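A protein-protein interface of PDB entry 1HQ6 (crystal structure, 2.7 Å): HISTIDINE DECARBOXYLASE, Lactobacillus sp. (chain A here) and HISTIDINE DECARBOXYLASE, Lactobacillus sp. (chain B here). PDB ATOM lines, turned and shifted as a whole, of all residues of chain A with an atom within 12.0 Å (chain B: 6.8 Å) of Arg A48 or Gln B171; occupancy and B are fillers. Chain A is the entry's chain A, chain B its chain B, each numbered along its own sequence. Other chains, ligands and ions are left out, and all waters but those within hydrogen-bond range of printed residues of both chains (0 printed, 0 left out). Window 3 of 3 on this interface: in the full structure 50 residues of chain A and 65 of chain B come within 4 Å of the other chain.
The backbone NH (N) of Gly B173 sits at hydrogen-bond distance from the backbone carbonyl oxygen (O) of Ala B78 (2.8 Å). The backbone NH (N) of Arg B80 is in hydrogen-bond range of the backbone carbonyl oxygen (O) of Gln B171 (3.2 Å). OE1 of Gln B171 is in hydrogen-bond range of N of Glu B168.
Among the printed residues, merely in contact across the chains: Val A47 with Ile B172 (3.1 Å), Ala A45 with Asn B174 (3.3 Å), Ala A65 with Asn B174 (3.3 Å), Arg A48 with Gln B171 (3.4 Å), Gly A46 with Gly B173 (3.5 Å), Glu A66 with Asn B174 (3.7 Å) and Val A47 with Gln B171 (3.9 Å).
Hydrophobic or aromatic side chains of chain A within 4 Å of the printed part of chain B: Ala A45, Val A47 and Ala A65. Along chain A the printed residues that touch a printed residue of chain B span positions 45 to 66. Of the 15 printed residues of chain B, 4 touch a printed residue of chain A. Hydrophobic or aromatic side chains of chain B within 4 Å of the printed part of chain A: Ile B172. Among the printed residues, no Asp or Glu carboxylate lies within 4 Å of a Lys or Arg side-chain nitrogen of the other chain.
The backbone NH of Asn B174 is in hydrogen-bond range of the backbone carbonyl oxygen of Gly A46 (2.8 Å). O of Arg A48 lies within hydrogen-bond range of N of Ile B172 (2.9 Å).
Of chain B, only Gln B171 and Ile B172 come within 4 Å of Arg A48. Gln B171 touches two residues of chain A. Ala B78 touches none of the printed residues of chain A. Glu B79 touches none of the printed residues of chain A. No residue of chain A comes within 4 Å of Pro B81. No residue of chain A comes within 4 Å of Met B167. No residue of chain A comes within 4 Å of Glu B168. No residue of chain A comes within 4 Å of Pro B169. No residue of chain A comes within 4 Å of Gly B170. Of chain A, only Val A47 and Arg A48 come within 4 Å of Ile B172. Gly B173 touches just one residue of chain A: Gly A46 (3.5 Å). Of the printed residues of chain B, Val A47 touches Gln B171 and Ile B172. Of the printed residues of chain B, Ala A65 touches Asn B174. The nearest residue of chain A that does not touch Gln B171 is Gly A46 (7.8 Å).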
ATOM      1  N   ASP A  44      19.708  22.687  -7.655  1.00  0.00           N
ATOM      2  CA  ASP A  44      19.495  21.265  -7.811  1.00  0.00           C
ATOM      3  C   ASP A  44      20.152  20.737  -9.073  1.00  0.00           C
ATOM      4  O   ASP A  44      20.200  21.415 -10.111  1.00  0.00           O
ATOM      5  CB  ASP A  44      18.018  20.964  -7.858  1.00  0.00           C
ATOM      6  CG  ASP A  44      17.630  20.317  -6.545  1.00  0.00           C
ATOM      7  OD1 ASP A  44      17.850  19.116  -6.401  1.00  0.00           O
ATOM      8  OD2 ASP A  44      17.139  21.005  -5.650  1.00  0.00           O
ATOM      9  N   ALA A  45      20.675  19.521  -9.015  1.00  0.00           N
ATOM     10  CA  ALA A  45      21.376  18.940 -10.145  1.00  0.00           C
ATOM     11  C   ALA A  45      20.880  17.531 -10.373  1.00  0.00           C
ATOM     12  O   ALA A  45      20.785  16.733  -9.439  1.00  0.00           O
ATOM     13  CB  ALA A  45      22.846  18.921  -9.838  1.00  0.00           C
ATOM     14  N   GLY A  46      20.566  17.202 -11.608  1.00  0.00           N
ATOM     15  CA  GLY A  46      19.964  15.932 -11.962  1.00  0.00           C
ATOM     16  C   GLY A  46      20.552  15.467 -13.287  1.00  0.00           C
ATOM     17  O   GLY A  46      21.156  16.243 -14.046  1.00  0.00           O
ATOM     18  N   VAL A  47      20.300  14.206 -13.629  1.00  0.00           N
ATOM     19  CA  VAL A  47      20.980  13.573 -14.748  1.00  0.00           C
ATOM     20  C   VAL A  47      19.968  12.715 -15.476  1.00  0.00           C
ATOM     21  O   VAL A  47      18.905  12.401 -14.909  1.00  0.00           O
ATOM     22  CB  VAL A  47      22.143  12.759 -14.123  1.00  0.00           C
ATOM     23  CG1 VAL A  47      21.611  11.548 -13.370  1.00  0.00           C
ATOM     24  CG2 VAL A  47      23.090  12.293 -15.194  1.00  0.00           C
ATOM     25  N   ARG A  48      20.250  12.422 -16.729  1.00  0.00           N
ATOM     26  CA  ARG A  48      19.487  11.396 -17.408  1.00  0.00           C
ATOM     27  C   ARG A  48      20.477  10.632 -18.285  1.00  0.00           C
ATOM     28  O   ARG A  48      21.292  11.266 -18.963  1.00  0.00           O
ATOM     29  CB  ARG A  48      18.309  11.996 -18.255  1.00  0.00           C
ATOM     30  CG  ARG A  48      18.388  13.099 -19.333  1.00  0.00           C
ATOM     31  CD  ARG A  48      16.963  13.222 -19.983  1.00  0.00           C
ATOM     32  NE  ARG A  48      16.684  14.502 -20.651  1.00  0.00           N
ATOM     33  CZ  ARG A  48      15.437  14.893 -21.021  1.00  0.00           C
ATOM     34  NH1 ARG A  48      15.257  16.093 -21.628  1.00  0.00           N
ATOM     35  NH2 ARG A  48      14.345  14.122 -20.799  1.00  0.00           N
ATOM     36  N   ARG A  64      13.643  17.706 -15.385  1.00  0.00           N
ATOM     37  CA  ARG A  64      14.742  16.871 -14.907  1.00  0.00           C
ATOM     38  C   ARG A  64      15.336  17.642 -13.734  1.00  0.00           C
ATOM     39  O   ARG A  64      14.695  17.497 -12.694  1.00  0.00           O
ATOM     40  CB  ARG A  64      15.779  16.628 -16.026  1.00  0.00           C
ATOM     41  CG  ARG A  64      15.240  15.905 -17.311  1.00  0.00           C
ATOM     42  CD  ARG A  64      14.228  14.714 -17.181  1.00  0.00           C
ATOM     43  NE  ARG A  64      14.531  13.818 -16.076  1.00  0.00           N
ATOM     44  CZ  ARG A  64      13.973  12.603 -15.913  1.00  0.00           C
ATOM     45  NH1 ARG A  64      14.341  11.859 -14.841  1.00  0.00           N
ATOM     46  NH2 ARG A  64      13.083  12.116 -16.801  1.00  0.00           N
ATOM     47  N   ALA A  65      16.377  18.501 -13.754  1.00  0.00           N
ATOM     48  CA  ALA A  65      16.800  19.240 -12.558  1.00  0.00           C
ATOM     49  C   ALA A  65      15.615  20.020 -11.970  1.00  0.00           C
ATOM     50  O   ALA A  65      15.245  19.778 -10.830  1.00  0.00           O
ATOM     51  CB  ALA A  65      17.903  20.223 -12.903  1.00  0.00           C
ATOM     52  N   GLU A  66      14.886  20.825 -12.771  1.00  0.00           N
ATOM     53  CA  GLU A  66      13.713  21.602 -12.323  1.00  0.00           C
ATOM     54  C   GLU A  66      12.615  20.821 -11.612  1.00  0.00           C
ATOM     55  O   GLU A  66      11.788  21.367 -10.873  1.00  0.00           O
ATOM     56  CB  GLU A  66      12.922  22.311 -13.442  1.00  0.00           C
ATOM     57  CG  GLU A  66      13.341  22.317 -14.901  1.00  0.00           C
ATOM     58  CD  GLU A  66      14.701  22.965 -15.132  1.00  0.00           C
ATOM     59  OE1 GLU A  66      15.623  22.283 -15.598  1.00  0.00           O
ATOM     60  OE2 GLU A  66      14.834  24.152 -14.844  1.00  0.00           O
ATOM     61  N   THR A  67      12.525  19.528 -11.869  1.00  0.00           N
ATOM     62  CA  THR A  67      11.460  18.773 -11.251  1.00  0.00           C
ATOM     63  C   THR A  67      11.930  18.059  -9.984  1.00  0.00           C
ATOM     64  O   THR A  67      11.124  17.418  -9.289  1.00  0.00           O
ATOM     65  CB  THR A  67      10.929  17.869 -12.403  1.00  0.00           C
ATOM     66  OG1 THR A  67      12.008  17.415 -13.243  1.00  0.00           O
ATOM     67  CG2 THR A  67       9.970  18.679 -13.269  1.00  0.00           C
ATOM     68  N   LYS A  68      13.227  18.159  -9.670  1.00  0.00           N
ATOM     69  CA  LYS A  68      13.773  17.509  -8.492  1.00  0.00           C
ATOM     70  C   LYS A  68      13.504  18.426  -7.319  1.00  0.00           C
ATOM     71  O   LYS A  68      13.676  19.641  -7.414  1.00  0.00           O
ATOM     72  CB  LYS A  68      15.304  17.337  -8.438  1.00  0.00           C
ATOM     73  CG  LYS A  68      16.019  16.376  -9.390  1.00  0.00           C
ATOM     74  CD  LYS A  68      17.541  16.321  -9.132  1.00  0.00           C
ATOM     75  CE  LYS A  68      18.012  15.395  -7.987  1.00  0.00           C
ATOM     76  NZ  LYS A  68      17.790  15.935  -6.647  1.00  0.00           N
ATOM     77  N   ALA B  78      25.723  19.280 -19.473  1.00  0.00           N
ATOM     78  CA  ALA B  78      26.929  18.732 -20.063  1.00  0.00           C
ATOM     79  C   ALA B  78      26.728  17.251 -20.186  1.00  0.00           C
ATOM     80  O   ALA B  78      25.946  16.657 -19.442  1.00  0.00           O
ATOM     81  CB  ALA B  78      28.146  18.964 -19.191  1.00  0.00           C
ATOM     82  N   GLU B  79      27.417  16.688 -21.158  1.00  0.00           N
ATOM     83  CA  GLU B  79      27.301  15.281 -21.505  1.00  0.00           C
ATOM     84  C   GLU B  79      28.607  14.564 -21.179  1.00  0.00           C
ATOM     85  O   GLU B  79      29.683  15.186 -21.104  1.00  0.00           O
ATOM     86  CB  GLU B  79      26.967  15.239 -23.004  1.00  0.00           C
ATOM     87  CG  GLU B  79      26.915  13.903 -23.744  1.00  0.00           C
ATOM     88  CD  GLU B  79      26.231  14.001 -25.107  1.00  0.00           C
ATOM     89  OE1 GLU B  79      26.676  14.795 -25.949  1.00  0.00           O
ATOM     90  OE2 GLU B  79      25.238  13.280 -25.308  1.00  0.00           O
ATOM     91  N   ARG B  80      28.483  13.257 -20.956  1.00  0.00           N
ATOM     92  CA  ARG B  80      29.632  12.375 -20.832  1.00  0.00           C
ATOM     93  C   ARG B  80      29.397  11.321 -21.918  1.00  0.00           C
ATOM     94  O   ARG B  80      28.398  10.592 -21.892  1.00  0.00           O
ATOM     95  CB  ARG B  80      29.675  11.733 -19.445  1.00  0.00           C
ATOM     96  CG  ARG B  80      30.772  10.666 -19.350  1.00  0.00           C
ATOM     97  CD  ARG B  80      31.505  10.634 -18.028  1.00  0.00           C
ATOM     98  NE  ARG B  80      31.062   9.619 -17.093  1.00  0.00           N
ATOM     99  CZ  ARG B  80      31.908   8.655 -16.680  1.00  0.00           C
ATOM    100  NH1 ARG B  80      31.485   7.746 -15.800  1.00  0.00           N
ATOM    101  NH2 ARG B  80      33.149   8.509 -17.165  1.00  0.00           N
ATOM    102  N   PRO B  81      30.237  11.203 -22.944  1.00  0.00           N
ATOM    103  CA  PRO B  81      30.014  10.327 -24.099  1.00  0.00           C
ATOM    104  C   PRO B  81      30.211   8.875 -23.688  1.00  0.00           C
ATOM    105  O   PRO B  81      30.700   8.619 -22.570  1.00  0.00           O
ATOM    106  CB  PRO B  81      31.014  10.838 -25.092  1.00  0.00           C
ATOM    107  CG  PRO B  81      32.195  11.155 -24.189  1.00  0.00           C
ATOM    108  CD  PRO B  81      31.545  11.849 -22.996  1.00  0.00           C
ATOM    109  N   LYS B  82      29.859   7.884 -24.524  1.00  0.00           N
ATOM    110  CA  LYS B  82      30.014   6.486 -24.104  1.00  0.00           C
ATOM    111  C   LYS B  82      31.494   6.140 -24.199  1.00  0.00           C
ATOM    112  O   LYS B  82      32.153   6.134 -25.241  1.00  0.00           O
ATOM    113  CB  LYS B  82      29.230   5.503 -24.971  1.00  0.00           C
ATOM    114  CG  LYS B  82      27.757   5.471 -24.580  1.00  0.00           C
ATOM    115  CD  LYS B  82      27.071   4.288 -25.288  1.00  0.00           C
ATOM    116  CE  LYS B  82      25.625   4.069 -24.814  1.00  0.00           C
ATOM    117  NZ  LYS B  82      25.575   3.579 -23.444  1.00  0.00           N
ATOM    118  N   GLY B  92      32.064  16.671 -20.096  1.00  0.00           N
ATOM    119  CA  GLY B  92      32.849  16.524 -18.887  1.00  0.00           C
ATOM    120  C   GLY B  92      32.302  15.335 -18.126  1.00  0.00           C
ATOM    121  O   GLY B  92      31.410  14.609 -18.609  1.00  0.00           O
ATOM    122  N   MET B 166      27.559  13.773 -10.699  1.00  0.00           N
ATOM    123  CA  MET B 166      28.617  13.175 -11.484  1.00  0.00           C
ATOM    124  C   MET B 166      27.834  12.405 -12.516  1.00  0.00           C
ATOM    125  O   MET B 166      26.825  11.778 -12.137  1.00  0.00           O
ATOM    126  CB  MET B 166      29.432  12.144 -10.740  1.00  0.00           C
ATOM    127  CG  MET B 166      30.247  12.623  -9.560  1.00  0.00           C
ATOM    128  SD  MET B 166      31.356  14.007  -9.947  1.00  0.00           S
ATOM    129  CE  MET B 166      32.241  13.381 -11.363  1.00  0.00           C
ATOM    130  N   MET B 167      28.254  12.417 -13.781  1.00  0.00           N
ATOM    131  CA  MET B 167      27.575  11.604 -14.778  1.00  0.00           C
ATOM    132  C   MET B 167      28.237  10.235 -14.842  1.00  0.00           C
ATOM    133  O   MET B 167      29.449  10.080 -14.562  1.00  0.00           O
ATOM    134  CB  MET B 167      27.663  12.169 -16.181  1.00  0.00           C
ATOM    135  CG  MET B 167      26.875  13.419 -16.369  1.00  0.00           C
ATOM    136  SD  MET B 167      27.718  14.770 -15.531  1.00  0.00           S
ATOM    137  CE  MET B 167      27.727  15.809 -16.954  1.00  0.00           C
ATOM    138  N   GLU B 168      27.437   9.210 -15.140  1.00  0.00           N
ATOM    139  CA  GLU B 168      28.038   7.915 -15.451  1.00  0.00           C
ATOM    140  C   GLU B 168      28.315   7.945 -16.973  1.00  0.00           C
ATOM    141  O   GLU B 168      27.912   8.948 -17.598  1.00  0.00           O
ATOM    142  CB  GLU B 168      27.046   6.829 -15.015  1.00  0.00           C
ATOM    143  CG  GLU B 168      27.524   6.035 -13.772  1.00  0.00           C
ATOM    144  CD  GLU B 168      27.594   6.761 -12.408  1.00  0.00           C
ATOM    145  OE1 GLU B 168      26.790   6.402 -11.513  1.00  0.00           O
ATOM    146  OE2 GLU B 168      28.456   7.650 -12.239  1.00  0.00           O
ATOM    147  N   PRO B 169      28.996   7.044 -17.719  1.00  0.00           N
ATOM    148  CA  PRO B 169      29.294   7.277 -19.130  1.00  0.00           C
ATOM    149  C   PRO B 169      27.996   7.229 -19.924  1.00  0.00           C
ATOM    150  O   PRO B 169      27.100   6.427 -19.637  1.00  0.00           O
ATOM    151  CB  PRO B 169      30.278   6.187 -19.499  1.00  0.00           C
ATOM    152  CG  PRO B 169      30.739   5.631 -18.158  1.00  0.00           C
ATOM    153  CD  PRO B 169      29.464   5.723 -17.322  1.00  0.00           C
ATOM    154  N   GLY B 170      27.863   8.117 -20.897  1.00  0.00           N
ATOM    155  CA  GLY B 170      26.690   8.114 -21.756  1.00  0.00           C
ATOM    156  C   GLY B 170      25.449   8.632 -21.040  1.00  0.00           C
ATOM    157  O   GLY B 170      24.355   8.102 -21.293  1.00  0.00           O
ATOM    158  N   GLN B 171      25.618   9.636 -20.155  1.00  0.00           N
ATOM    159  CA  GLN B 171      24.526  10.312 -19.423  1.00  0.00           C
ATOM    160  C   GLN B 171      24.768  11.813 -19.377  1.00  0.00           C
ATOM    161  O   GLN B 171      25.928  12.230 -19.239  1.00  0.00           O
ATOM    162  CB  GLN B 171      24.409   9.883 -17.964  1.00  0.00           C
ATOM    163  CG  GLN B 171      23.684   8.566 -17.764  1.00  0.00           C
ATOM    164  CD  GLN B 171      23.320   8.313 -16.314  1.00  0.00           C
ATOM    165  OE1 GLN B 171      24.118   8.524 -15.387  1.00  0.00           O
ATOM    166  NE2 GLN B 171      22.085   7.897 -16.080  1.00  0.00           N
ATOM    167  N   ILE B 172      23.741  12.656 -19.508  1.00  0.00           N
ATOM    168  CA  ILE B 172      23.885  14.108 -19.446  1.00  0.00           C
ATOM    169  C   ILE B 172      23.397  14.621 -18.091  1.00  0.00           C
ATOM    170  O   ILE B 172      22.390  14.180 -17.508  1.00  0.00           O
ATOM    171  CB  ILE B 172      23.072  14.875 -20.545  1.00  0.00           C
ATOM    172  CG1 ILE B 172      21.577  14.611 -20.465  1.00  0.00           C
ATOM    173  CG2 ILE B 172      23.543  14.413 -21.904  1.00  0.00           C
ATOM    174  CD1 ILE B 172      20.752  15.910 -20.323  1.00  0.00           C
ATOM    175  N   GLY B 173      24.131  15.594 -17.585  1.00  0.00           N
ATOM    176  CA  GLY B 173      23.816  16.180 -16.310  1.00  0.00           C
ATOM    177  C   GLY B 173      23.431  17.609 -16.557  1.00  0.00           C
ATOM    178  O   GLY B 173      23.950  18.298 -17.453  1.00  0.00           O
ATOM    179  N   ASN B 174      22.452  18.000 -15.773  1.00  0.00           N
ATOM    180  CA  ASN B 174      21.896  19.343 -15.811  1.00  0.00           C
ATOM    181  C   ASN B 174      21.970  19.857 -14.391  1.00  0.00           C
ATOM    182  O   ASN B 174      21.708  19.108 -13.440  1.00  0.00           O
ATOM    183  CB  ASN B 174      20.449  19.289 -16.270  1.00  0.00           C
ATOM    184  CG  ASN B 174      19.893  20.667 -16.616  1.00  0.00           C
ATOM    185  OD1 ASN B 174      19.121  21.238 -15.846  1.00  0.00           O
ATOM    186  ND2 ASN B 174      20.199  21.213 -17.800  1.00  0.00           N
